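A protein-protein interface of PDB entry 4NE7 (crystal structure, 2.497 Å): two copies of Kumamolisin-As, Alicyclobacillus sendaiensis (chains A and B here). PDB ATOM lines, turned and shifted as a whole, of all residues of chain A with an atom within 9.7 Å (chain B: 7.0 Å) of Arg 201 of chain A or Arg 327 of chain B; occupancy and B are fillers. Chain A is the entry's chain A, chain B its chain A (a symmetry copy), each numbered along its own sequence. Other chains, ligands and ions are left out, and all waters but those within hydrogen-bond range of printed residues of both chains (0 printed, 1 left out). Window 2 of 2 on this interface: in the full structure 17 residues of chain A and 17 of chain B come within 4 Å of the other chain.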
ATOM      1  N   TYR A   6      -0.916   5.368  11.947  1.00  0.00           N
ATOM      2  CA  TYR A   6      -1.834   4.649  11.071  1.00  0.00           C
ATOM      3  C   TYR A   6      -3.277   5.124  11.185  1.00  0.00           C
ATOM      4  O   TYR A   6      -3.661   5.780  12.152  1.00  0.00           O
ATOM      5  CB  TYR A   6      -1.781   3.149  11.363  1.00  0.00           C
ATOM      6  CG  TYR A   6      -0.390   2.569  11.321  1.00  0.00           C
ATOM      7  CD1 TYR A   6       0.278   2.404  10.114  1.00  0.00           C
ATOM      8  CD2 TYR A   6       0.256   2.184  12.485  1.00  0.00           C
ATOM      9  CE1 TYR A   6       1.549   1.878  10.069  1.00  0.00           C
ATOM     10  CE2 TYR A   6       1.532   1.654  12.451  1.00  0.00           C
ATOM     11  CZ  TYR A   6       2.172   1.503  11.240  1.00  0.00           C
ATOM     12  OH  TYR A   6       3.442   0.975  11.197  1.00  0.00           O
ATOM     13  N   LEU A   9      -7.998   1.605   9.303  1.00  0.00           N
ATOM     14  CA  LEU A   9      -7.973   0.755   8.117  1.00  0.00           C
ATOM     15  C   LEU A   9      -6.596   0.124   7.896  1.00  0.00           C
ATOM     16  O   LEU A   9      -6.497  -1.052   7.541  1.00  0.00           O
ATOM     17  CB  LEU A   9      -8.387   1.552   6.877  1.00  0.00           C
ATOM     18  CG  LEU A   9      -9.577   2.508   6.996  1.00  0.00           C
ATOM     19  CD1 LEU A   9      -9.831   3.205   5.667  1.00  0.00           C
ATOM     20  CD2 LEU A   9     -10.833   1.791   7.474  1.00  0.00           C
ATOM     21  N   ASP A  10      -5.538   0.907   8.102  1.00  0.00           N
ATOM     22  CA  ASP A  10      -4.172   0.402   7.959  1.00  0.00           C
ATOM     23  C   ASP A  10      -3.890  -0.730   8.936  1.00  0.00           C
ATOM     24  O   ASP A  10      -3.335  -1.766   8.564  1.00  0.00           O
ATOM     25  CB  ASP A  10      -3.148   1.519   8.169  1.00  0.00           C
ATOM     26  CG  ASP A  10      -3.154   2.541   7.047  1.00  0.00           C
ATOM     27  OD1 ASP A  10      -3.397   2.152   5.881  1.00  0.00           O
ATOM     28  OD2 ASP A  10      -2.914   3.734   7.335  1.00  0.00           O
ATOM     29  N   VAL A  11      -4.266  -0.517  10.192  1.00  0.00           N
ATOM     30  CA  VAL A  11      -4.052  -1.511  11.234  1.00  0.00           C
ATOM     31  C   VAL A  11      -4.866  -2.766  10.938  1.00  0.00           C
ATOM     32  O   VAL A  11      -4.389  -3.888  11.118  1.00  0.00           O
ATOM     33  CB  VAL A  11      -4.428  -0.960  12.620  1.00  0.00           C
ATOM     34  CG1 VAL A  11      -4.204  -2.016  13.686  1.00  0.00           C
ATOM     35  CG2 VAL A  11      -3.617   0.297  12.923  1.00  0.00           C
ATOM     36  N   ALA A  12      -6.092  -2.562  10.463  1.00  0.00           N
ATOM     37  CA  ALA A  12      -6.989  -3.664  10.134  1.00  0.00           C
ATOM     38  C   ALA A  12      -6.429  -4.539   9.012  1.00  0.00           C
ATOM     39  O   ALA A  12      -6.582  -5.760   9.036  1.00  0.00           O
ATOM     40  CB  ALA A  12      -8.365  -3.131   9.763  1.00  0.00           C
ATOM     41  N   GLN A  13      -5.784  -3.911   8.033  1.00  0.00           N
ATOM     42  CA  GLN A  13      -5.171  -4.655   6.937  1.00  0.00           C
ATOM     43  C   GLN A  13      -3.997  -5.484   7.435  1.00  0.00           C
ATOM     44  O   GLN A  13      -3.826  -6.636   7.034  1.00  0.00           O
ATOM     45  CB  GLN A  13      -4.725  -3.715   5.816  1.00  0.00           C
ATOM     46  CG  GLN A  13      -5.867  -3.226   4.944  1.00  0.00           C
ATOM     47  CD  GLN A  13      -5.434  -2.155   3.962  1.00  0.00           C
ATOM     48  OE1 GLN A  13      -4.263  -2.071   3.591  1.00  0.00           O
ATOM     49  NE2 GLN A  13      -6.380  -1.321   3.544  1.00  0.00           N
ATOM     50  N   ALA A  14      -3.196  -4.893   8.317  1.00  0.00           N
ATOM     51  CA  ALA A  14      -2.063  -5.589   8.918  1.00  0.00           C
ATOM     52  C   ALA A  14      -2.514  -6.813   9.711  1.00  0.00           C
ATOM     53  O   ALA A  14      -1.880  -7.868   9.660  1.00  0.00           O
ATOM     54  CB  ALA A  14      -1.277  -4.642   9.804  1.00  0.00           C
ATOM     55  N   TYR A  15      -3.616  -6.671  10.441  1.00  0.00           N
ATOM     56  CA  TYR A  15      -4.156  -7.785  11.214  1.00  0.00           C
ATOM     57  C   TYR A  15      -5.070  -8.646  10.354  1.00  0.00           C
ATOM     58  O   TYR A  15      -5.662  -9.616  10.838  1.00  0.00           O
ATOM     59  CB  TYR A  15      -4.898  -7.289  12.456  1.00  0.00           C
ATOM     60  CG  TYR A  15      -4.002  -6.619  13.473  1.00  0.00           C
ATOM     61  CD1 TYR A  15      -2.652  -6.941  13.554  1.00  0.00           C
ATOM     62  CD2 TYR A  15      -4.503  -5.664  14.347  1.00  0.00           C
ATOM     63  CE1 TYR A  15      -1.826  -6.330  14.480  1.00  0.00           C
ATOM     64  CE2 TYR A  15      -3.685  -5.050  15.279  1.00  0.00           C
ATOM     65  CZ  TYR A  15      -2.347  -5.385  15.340  1.00  0.00           C
ATOM     66  OH  TYR A  15      -1.529  -4.771  16.264  1.00  0.00           O
ATOM     67  N   GLN A  16      -5.181  -8.275   9.079  1.00  0.00           N
ATOM     68  CA  GLN A  16      -5.932  -9.047   8.090  1.00  0.00           C
ATOM     69  C   GLN A  16      -7.397  -9.281   8.459  1.00  0.00           C
ATOM     70  O   GLN A  16      -7.867 -10.418   8.461  1.00  0.00           O
ATOM     71  CB  GLN A  16      -5.222 -10.373   7.785  1.00  0.00           C
ATOM     72  CG  GLN A  16      -4.041 -10.212   6.829  1.00  0.00           C
ATOM     73  CD  GLN A  16      -3.086 -11.393   6.857  1.00  0.00           C
ATOM     74  OE1 GLN A  16      -3.465 -12.531   6.569  1.00  0.00           O
ATOM     75  NE2 GLN A  16      -1.833 -11.125   7.204  1.00  0.00           N
ATOM     76  N   LEU A 195       3.212  -1.614  16.773  1.00  0.00           N
ATOM     77  CA  LEU A 195       3.069  -2.213  15.454  1.00  0.00           C
ATOM     78  C   LEU A 195       3.840  -1.458  14.380  1.00  0.00           C
ATOM     79  O   LEU A 195       3.683  -0.247  14.222  1.00  0.00           O
ATOM     80  CB  LEU A 195       1.593  -2.291  15.064  1.00  0.00           C
ATOM     81  CG  LEU A 195       1.295  -2.895  13.691  1.00  0.00           C
ATOM     82  CD1 LEU A 195       1.545  -4.400  13.691  1.00  0.00           C
ATOM     83  CD2 LEU A 195      -0.129  -2.581  13.276  1.00  0.00           C
ATOM     84  N   VAL A 196       4.676  -2.188  13.650  1.00  0.00           N
ATOM     85  CA  VAL A 196       5.315  -1.662  12.452  1.00  0.00           C
ATOM     86  C   VAL A 196       4.821  -2.454  11.245  1.00  0.00           C
ATOM     87  O   VAL A 196       5.195  -3.614  11.048  1.00  0.00           O
ATOM     88  CB  VAL A 196       6.851  -1.731  12.542  1.00  0.00           C
ATOM     89  CG1 VAL A 196       7.485  -1.253  11.245  1.00  0.00           C
ATOM     90  CG2 VAL A 196       7.346  -0.901  13.709  1.00  0.00           C
ATOM     91  N   ALA A 197       3.958  -1.829  10.454  1.00  0.00           N
ATOM     92  CA  ALA A 197       3.400  -2.465   9.270  1.00  0.00           C
ATOM     93  C   ALA A 197       3.530  -1.532   8.075  1.00  0.00           C
ATOM     94  O   ALA A 197       3.390  -0.315   8.211  1.00  0.00           O
ATOM     95  CB  ALA A 197       1.948  -2.830   9.504  1.00  0.00           C
ATOM     96  N   SER A 198       3.804  -2.100   6.907  1.00  0.00           N
ATOM     97  CA  SER A 198       3.986  -1.297   5.702  1.00  0.00           C
ATOM     98  C   SER A 198       3.382  -1.968   4.473  1.00  0.00           C
ATOM     99  O   SER A 198       4.084  -2.629   3.708  1.00  0.00           O
ATOM    100  CB  SER A 198       5.470  -1.002   5.470  1.00  0.00           C
ATOM    101  OG  SER A 198       6.211  -2.201   5.337  1.00  0.00           O
ATOM    102  N   GLY A 199       2.075  -1.800   4.295  1.00  0.00           N
ATOM    103  CA  GLY A 199       1.388  -2.342   3.139  1.00  0.00           C
ATOM    104  C   GLY A 199       0.714  -3.676   3.399  1.00  0.00           C
ATOM    105  O   GLY A 199       1.015  -4.671   2.740  1.00  0.00           O
ATOM    106  N   GLY A 200      -0.192  -3.699   4.371  1.00  0.00           N
ATOM    107  CA  GLY A 200      -0.991  -4.879   4.655  1.00  0.00           C
ATOM    108  C   GLY A 200      -0.245  -6.030   5.303  1.00  0.00           C
ATOM    109  O   GLY A 200      -0.829  -7.087   5.553  1.00  0.00           O
ATOM    110  N   ARG A 201       1.043  -5.834   5.572  1.00  0.00           N
ATOM    111  CA  ARG A 201       1.853  -6.867   6.212  1.00  0.00           C
ATOM    112  C   ARG A 201       2.570  -6.349   7.452  1.00  0.00           C
ATOM    113  O   ARG A 201       2.961  -5.185   7.525  1.00  0.00           O
ATOM    114  CB  ARG A 201       2.866  -7.454   5.230  1.00  0.00           C
ATOM    115  CG  ARG A 201       2.235  -8.229   4.090  1.00  0.00           C
ATOM    116  CD  ARG A 201       3.287  -8.830   3.179  1.00  0.00           C
ATOM    117  NE  ARG A 201       2.691  -9.496   2.024  1.00  0.00           N
ATOM    118  CZ  ARG A 201       2.387  -8.882   0.885  1.00  0.00           C
ATOM    119  NH1 ARG A 201       2.618  -7.582   0.746  1.00  0.00           N
ATOM    120  NH2 ARG A 201       1.849  -9.566  -0.117  1.00  0.00           N
ATOM    121  N   ILE A 202       2.738  -7.232   8.428  1.00  0.00           N
ATOM    122  CA  ILE A 202       3.436  -6.892   9.656  1.00  0.00           C
ATOM    123  C   ILE A 202       4.947  -7.044   9.486  1.00  0.00           C
ATOM    124  O   ILE A 202       5.456  -8.153   9.324  1.00  0.00           O
ATOM    125  CB  ILE A 202       2.958  -7.770  10.831  1.00  0.00           C
ATOM    126  CG1 ILE A 202       1.470  -7.542  11.090  1.00  0.00           C
ATOM    127  CG2 ILE A 202       3.766  -7.473  12.080  1.00  0.00           C
ATOM    128  CD1 ILE A 202       0.912  -8.357  12.239  1.00  0.00           C
ATOM    129  N   ALA A 203       5.658  -5.921   9.508  1.00  0.00           N
ATOM    130  CA  ALA A 203       7.113  -5.944   9.461  1.00  0.00           C
ATOM    131  C   ALA A 203       7.641  -6.476  10.788  1.00  0.00           C
ATOM    132  O   ALA A 203       8.408  -7.436  10.824  1.00  0.00           O
ATOM    133  CB  ALA A 203       7.661  -4.554   9.184  1.00  0.00           C
ATOM    134  N   GLN A 204       7.228  -5.838  11.879  1.00  0.00           N
ATOM    135  CA  GLN A 204       7.514  -6.352  13.212  1.00  0.00           C
ATOM    136  C   GLN A 204       6.510  -5.851  14.241  1.00  0.00           C
ATOM    137  O   GLN A 204       5.986  -4.742  14.127  1.00  0.00           O
ATOM    138  CB  GLN A 204       8.946  -6.020  13.642  1.00  0.00           C
ATOM    139  CG  GLN A 204       9.215  -4.559  13.918  1.00  0.00           C
ATOM    140  CD  GLN A 204      10.695  -4.270  14.103  1.00  0.00           C
ATOM    141  OE1 GLN A 204      11.529  -4.692  13.294  1.00  0.00           O
ATOM    142  NE2 GLN A 204      11.030  -3.538  15.165  1.00  0.00           N
ATOM    143  N   GLU A 205       6.235  -6.684  15.238  1.00  0.00           N
ATOM    144  CA  GLU A 205       5.328  -6.300  16.313  1.00  0.00           C
ATOM    145  C   GLU A 205       5.900  -6.702  17.667  1.00  0.00           C
ATOM    146  O   GLU A 205       6.249  -7.862  17.885  1.00  0.00           O
ATOM    147  CB  GLU A 205       3.947  -6.923  16.106  1.00  0.00           C
ATOM    148  CG  GLU A 205       2.837  -6.209  16.856  1.00  0.00           C
ATOM    149  CD  GLU A 205       1.479  -6.862  16.664  1.00  0.00           C
ATOM    150  OE1 GLU A 205       1.413  -7.945  16.040  1.00  0.00           O
ATOM    151  OE2 GLU A 205       0.477  -6.284  17.140  1.00  0.00           O
ATOM    152  N   HIS A 315      -0.676 -13.805  15.499  1.00  0.00           N
ATOM    153  CA  HIS A 315       0.717 -13.404  15.380  1.00  0.00           C
ATOM    154  C   HIS A 315       1.353 -13.363  16.764  1.00  0.00           C
ATOM    155  O   HIS A 315       1.175 -12.401  17.506  1.00  0.00           O
ATOM    156  CB  HIS A 315       0.853 -12.035  14.724  1.00  0.00           C
ATOM    157  CG  HIS A 315       2.254 -11.509  14.726  1.00  0.00           C
ATOM    158  ND1 HIS A 315       2.548 -10.164  14.790  1.00  0.00           N
ATOM    159  CD2 HIS A 315       3.447 -12.153  14.679  1.00  0.00           C
ATOM    160  CE1 HIS A 315       3.858 -10.003  14.780  1.00  0.00           C
ATOM    161  NE2 HIS A 315       4.428 -11.191  14.715  1.00  0.00           N
ATOM    162  N   ILE A 347      -5.154 -12.773  13.532  1.00  0.00           N
ATOM    163  CA  ILE A 347      -5.162 -12.661  12.082  1.00  0.00           C
ATOM    164  C   ILE A 347      -6.585 -12.942  11.623  1.00  0.00           C
ATOM    165  O   ILE A 347      -7.008 -14.097  11.560  1.00  0.00           O
ATOM    166  CB  ILE A 347      -4.190 -13.656  11.433  1.00  0.00           C
ATOM    167  CG1 ILE A 347      -2.797 -13.510  12.055  1.00  0.00           C
ATOM    168  CG2 ILE A 347      -4.141 -13.450   9.923  1.00  0.00           C
ATOM    169  CD1 ILE A 347      -1.786 -14.505  11.534  1.00  0.00           C
ATOM    170  N   TYR B 176      17.995 -11.669  -4.773  1.00  0.00           N
ATOM    171  CA  TYR B 176      18.643 -11.330  -3.508  1.00  0.00           C
ATOM    172  C   TYR B 176      20.158 -11.528  -3.568  1.00  0.00           C
ATOM    173  O   TYR B 176      20.647 -12.484  -4.172  1.00  0.00           O
ATOM    174  CB  TYR B 176      18.036 -12.152  -2.367  1.00  0.00           C
ATOM    175  CG  TYR B 176      16.534 -12.006  -2.267  1.00  0.00           C
ATOM    176  CD1 TYR B 176      15.963 -10.832  -1.790  1.00  0.00           C
ATOM    177  CD2 TYR B 176      15.687 -13.038  -2.656  1.00  0.00           C
ATOM    178  CE1 TYR B 176      14.593 -10.688  -1.703  1.00  0.00           C
ATOM    179  CE2 TYR B 176      14.315 -12.903  -2.572  1.00  0.00           C
ATOM    180  CZ  TYR B 176      13.772 -11.726  -2.095  1.00  0.00           C
ATOM    181  OH  TYR B 176      12.405 -11.583  -2.006  1.00  0.00           O
ATOM    182  N   PRO B 212      10.579   1.367   3.011  1.00  0.00           N
ATOM    183  CA  PRO B 212      11.294   1.086   1.760  1.00  0.00           C
ATOM    184  C   PRO B 212      12.265   2.195   1.359  1.00  0.00           C
ATOM    185  O   PRO B 212      12.572   2.325   0.175  1.00  0.00           O
ATOM    186  CB  PRO B 212      10.161   0.997   0.723  1.00  0.00           C
ATOM    187  CG  PRO B 212       8.872   0.998   1.516  1.00  0.00           C
ATOM    188  CD  PRO B 212       9.185   1.753   2.759  1.00  0.00           C
ATOM    189  N   ASN B 321      12.220  -8.607   9.515  1.00  0.00           N
ATOM    190  CA  ASN B 321      12.664  -9.200   8.257  1.00  0.00           C
ATOM    191  C   ASN B 321      13.643  -8.307   7.493  1.00  0.00           C
ATOM    192  O   ASN B 321      13.749  -7.109   7.773  1.00  0.00           O
ATOM    193  CB  ASN B 321      11.468  -9.556   7.368  1.00  0.00           C
ATOM    194  CG  ASN B 321      10.661  -8.338   6.962  1.00  0.00           C
ATOM    195  OD1 ASN B 321      11.068  -7.572   6.087  1.00  0.00           O
ATOM    196  ND2 ASN B 321       9.507  -8.156   7.594  1.00  0.00           N
ATOM    197  N   ASP B 323      13.556  -7.789   4.181  1.00  0.00           N
ATOM    198  CA  ASP B 323      12.933  -7.248   2.979  1.00  0.00           C
ATOM    199  C   ASP B 323      12.681  -5.752   3.120  1.00  0.00           C
ATOM    200  O   ASP B 323      11.874  -5.323   3.948  1.00  0.00           O
ATOM    201  CB  ASP B 323      11.625  -7.985   2.685  1.00  0.00           C
ATOM    202  CG  ASP B 323      11.148  -7.791   1.258  1.00  0.00           C
ATOM    203  OD1 ASP B 323      11.160  -6.643   0.769  1.00  0.00           O
ATOM    204  OD2 ASP B 323      10.763  -8.793   0.621  1.00  0.00           O
ATOM    205  N   ILE B 324      13.375  -4.963   2.308  1.00  0.00           N
ATOM    206  CA  ILE B 324      13.220  -3.516   2.342  1.00  0.00           C
ATOM    207  C   ILE B 324      11.848  -3.111   1.792  1.00  0.00           C
ATOM    208  O   ILE B 324      11.286  -2.091   2.190  1.00  0.00           O
ATOM    209  CB  ILE B 324      14.375  -2.800   1.591  1.00  0.00           C
ATOM    210  CG1 ILE B 324      14.288  -1.283   1.773  1.00  0.00           C
ATOM    211  CG2 ILE B 324      14.389  -3.182   0.116  1.00  0.00           C
ATOM    212  CD1 ILE B 324      15.431  -0.525   1.135  1.00  0.00           C
ATOM    213  N   ALA B 325      11.300  -3.934   0.901  1.00  0.00           N
ATOM    214  CA  ALA B 325       9.980  -3.677   0.327  1.00  0.00           C
ATOM    215  C   ALA B 325       8.852  -4.209   1.215  1.00  0.00           C
ATOM    216  O   ALA B 325       7.694  -3.815   1.061  1.00  0.00           O
ATOM    217  CB  ALA B 325       9.883  -4.278  -1.071  1.00  0.00           C
ATOM    218  N   ASN B 326       9.201  -5.103   2.137  1.00  0.00           N
ATOM    219  CA  ASN B 326       8.235  -5.747   3.025  1.00  0.00           C
ATOM    220  C   ASN B 326       7.107  -6.446   2.256  1.00  0.00           C
ATOM    221  O   ASN B 326       5.936  -6.379   2.638  1.00  0.00           O
ATOM    222  CB  ASN B 326       7.673  -4.747   4.045  1.00  0.00           C
ATOM    223  CG  ASN B 326       6.980  -5.426   5.217  1.00  0.00           C
ATOM    224  OD1 ASN B 326       7.257  -6.585   5.536  1.00  0.00           O
ATOM    225  ND2 ASN B 326       6.071  -4.705   5.862  1.00  0.00           N
ATOM    226  N   ARG B 327       7.478  -7.115   1.168  1.00  0.00           N
ATOM    227  CA  ARG B 327       6.525  -7.873   0.364  1.00  0.00           C
ATOM    228  C   ARG B 327       6.684  -9.365   0.608  1.00  0.00           C
ATOM    229  O   ARG B 327       5.897  -9.972   1.334  1.00  0.00           O
ATOM    230  CB  ARG B 327       6.713  -7.558  -1.119  1.00  0.00           C
ATOM    231  CG  ARG B 327       5.951  -6.338  -1.587  1.00  0.00           C
ATOM    232  CD  ARG B 327       6.610  -5.701  -2.800  1.00  0.00           C
ATOM    233  NE  ARG B 327       5.776  -4.655  -3.386  1.00  0.00           N
ATOM    234  CZ  ARG B 327       5.599  -3.449  -2.856  1.00  0.00           C
ATOM    235  NH1 ARG B 327       6.193  -3.126  -1.713  1.00  0.00           N
ATOM    236  NH2 ARG B 327       4.821  -2.564  -3.467  1.00  0.00           N
ATOM    237  N   ALA B 328       7.708  -9.956   0.003  1.00  0.00           N
ATOM    238  CA  ALA B 328       7.979 -11.378   0.176  1.00  0.00           C
ATOM    239  C   ALA B 328       8.472 -11.667   1.587  1.00  0.00           C
ATOM    240  O   ALA B 328       8.443 -12.811   2.040  1.00  0.00           O
ATOM    241  CB  ALA B 328       9.000 -11.848  -0.845  1.00  0.00           C
ATOM    242  N   GLN B 329       8.931 -10.618   2.266  1.00  0.00           N
ATOM    243  CA  GLN B 329       9.457 -10.716   3.625  1.00  0.00           C
ATOM    244  C   GLN B 329      10.644 -11.671   3.705  1.00  0.00           C
ATOM    245  O   GLN B 329      10.706 -12.548   4.568  1.00  0.00           O
ATOM    246  CB  GLN B 329       8.356 -11.113   4.608  1.00  0.00           C
ATOM    247  CG  GLN B 329       7.155 -10.189   4.562  1.00  0.00           C
ATOM    248  CD  GLN B 329       6.217 -10.401   5.729  1.00  0.00           C
ATOM    249  OE1 GLN B 329       5.765 -11.519   5.984  1.00  0.00           O
ATOM    250  NE2 GLN B 329       5.926  -9.329   6.455  1.00  0.00           N
ATOM    251  N   ILE B 330      11.587 -11.487   2.790  1.00  0.00           N
ATOM    252  CA  ILE B 330      12.787 -12.304   2.742  1.00  0.00           C
ATOM    253  C   ILE B 330      13.988 -11.405   3.011  1.00  0.00           C
ATOM    254  O   ILE B 330      14.129 -10.361   2.376  1.00  0.00           O
ATOM    255  CB  ILE B 330      12.928 -12.981   1.366  1.00  0.00           C
ATOM    256  CG1 ILE B 330      11.798 -13.991   1.157  1.00  0.00           C
ATOM    257  CG2 ILE B 330      14.279 -13.662   1.228  1.00  0.00           C
ATOM    258  CD1 ILE B 330      11.801 -14.640  -0.213  1.00  0.00           C
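Of the printed residues of chain B, Ser 198 of chain A touches Asn 326.
No residue of chain B comes within 4 Å of Gly 200 of chain A.
Of chain B, only Asn 326, Arg 327 and Gln 329 come within 4 Å of Arg 201 of chain A.
Ile 347 of chain A touches none of the printed residues of chain B.
No residue of chain A comes within 4 Å of Ala 325 of chain B.
Arg 327 of chain B touches one residue of chain A.
No residue of chain A comes within 4 Å of Ala 328 of chain B.
Printed residues of chain A within 4 Å of Gln 329 of chain B: Arg 201 and Ile 202.
The nearest residue of chain B that does not touch Arg 201 of chain A is Ala 328 of chain B (5.4 Å).
The nearest residue of chain A that does not touch Arg 327 of chain B is Ser 198 of chain A (5.8 Å).
The nearest printed residue of chain A that does not touch Gln 329 of chain B is Ala 203 of chain A (4.6 Å).
No position is printed for both chains.
Of the 7 pairs that touch across the chains among the printed residues, none has its exchanged pair printed and touching as well.
Of the 11 printed residues of chain B, 4 touch a printed residue of chain A.
Along chain B the printed residues that touch a printed residue of chain A span positions 321 to 329.
Among the printed residues, 7 pairs touch across the chains.
ND2 of Asn 321 of chain B sits at hydrogen-bond distance from OD1 of Asn 326 of chain B (3.4 Å).
N of Gln 329 of chain B is in hydrogen-bond range of OD2 of Asp 323 of chain B, at 3.1 Å.
OD1 of Asp 323 of chain B sits at hydrogen-bond distance from N of Asn 326 of chain B (2.8 Å).
OD1 of Asn 326 of chain B lies within hydrogen-bond range of NE2 of Gln 329 of chain B (3.2 Å).
The side-chain amide oxygen (OD1) of Asn 321 of chain B lies within hydrogen-bond range of the backbone NH (N) of Asp 323 of chain B, 3.1 Å away.
The backbone carbonyl oxygen of Val 196 of chain A lies within hydrogen-bond range of the backbone NH of Ala 203 of chain A (2.8 Å).
Among the printed residues, merely in contact across the chains: Arg 201 of chain A with Asn 326 of chain B, Arg 201 of chain A with Gln 329 of chain B and Ala 203 of chain A with Asn 326 of chain B.
The side-chain amide nitrogen (ND2) of Asn 326 of chain B sits at hydrogen-bond distance from the side-chain hydroxyl (OG) of Ser 198 of chain A, 2.6 Å away.
The backbone carbonyl oxygen of Ile 202 of chain A lies within hydrogen-bond range of the side-chain amide nitrogen of Gln 329 of chain B, at 3.1 Å.
The backbone carbonyl oxygen (O) of Arg 327 of chain B sits at hydrogen-bond distance from the guanidinium group (NE) of Arg 201 of chain A, 3.3 Å away.
The backbone carbonyl oxygen of Ala 203 of chain A sits at hydrogen-bond distance from the side-chain amide nitrogen of Asn 321 of chain B (3.5 Å).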
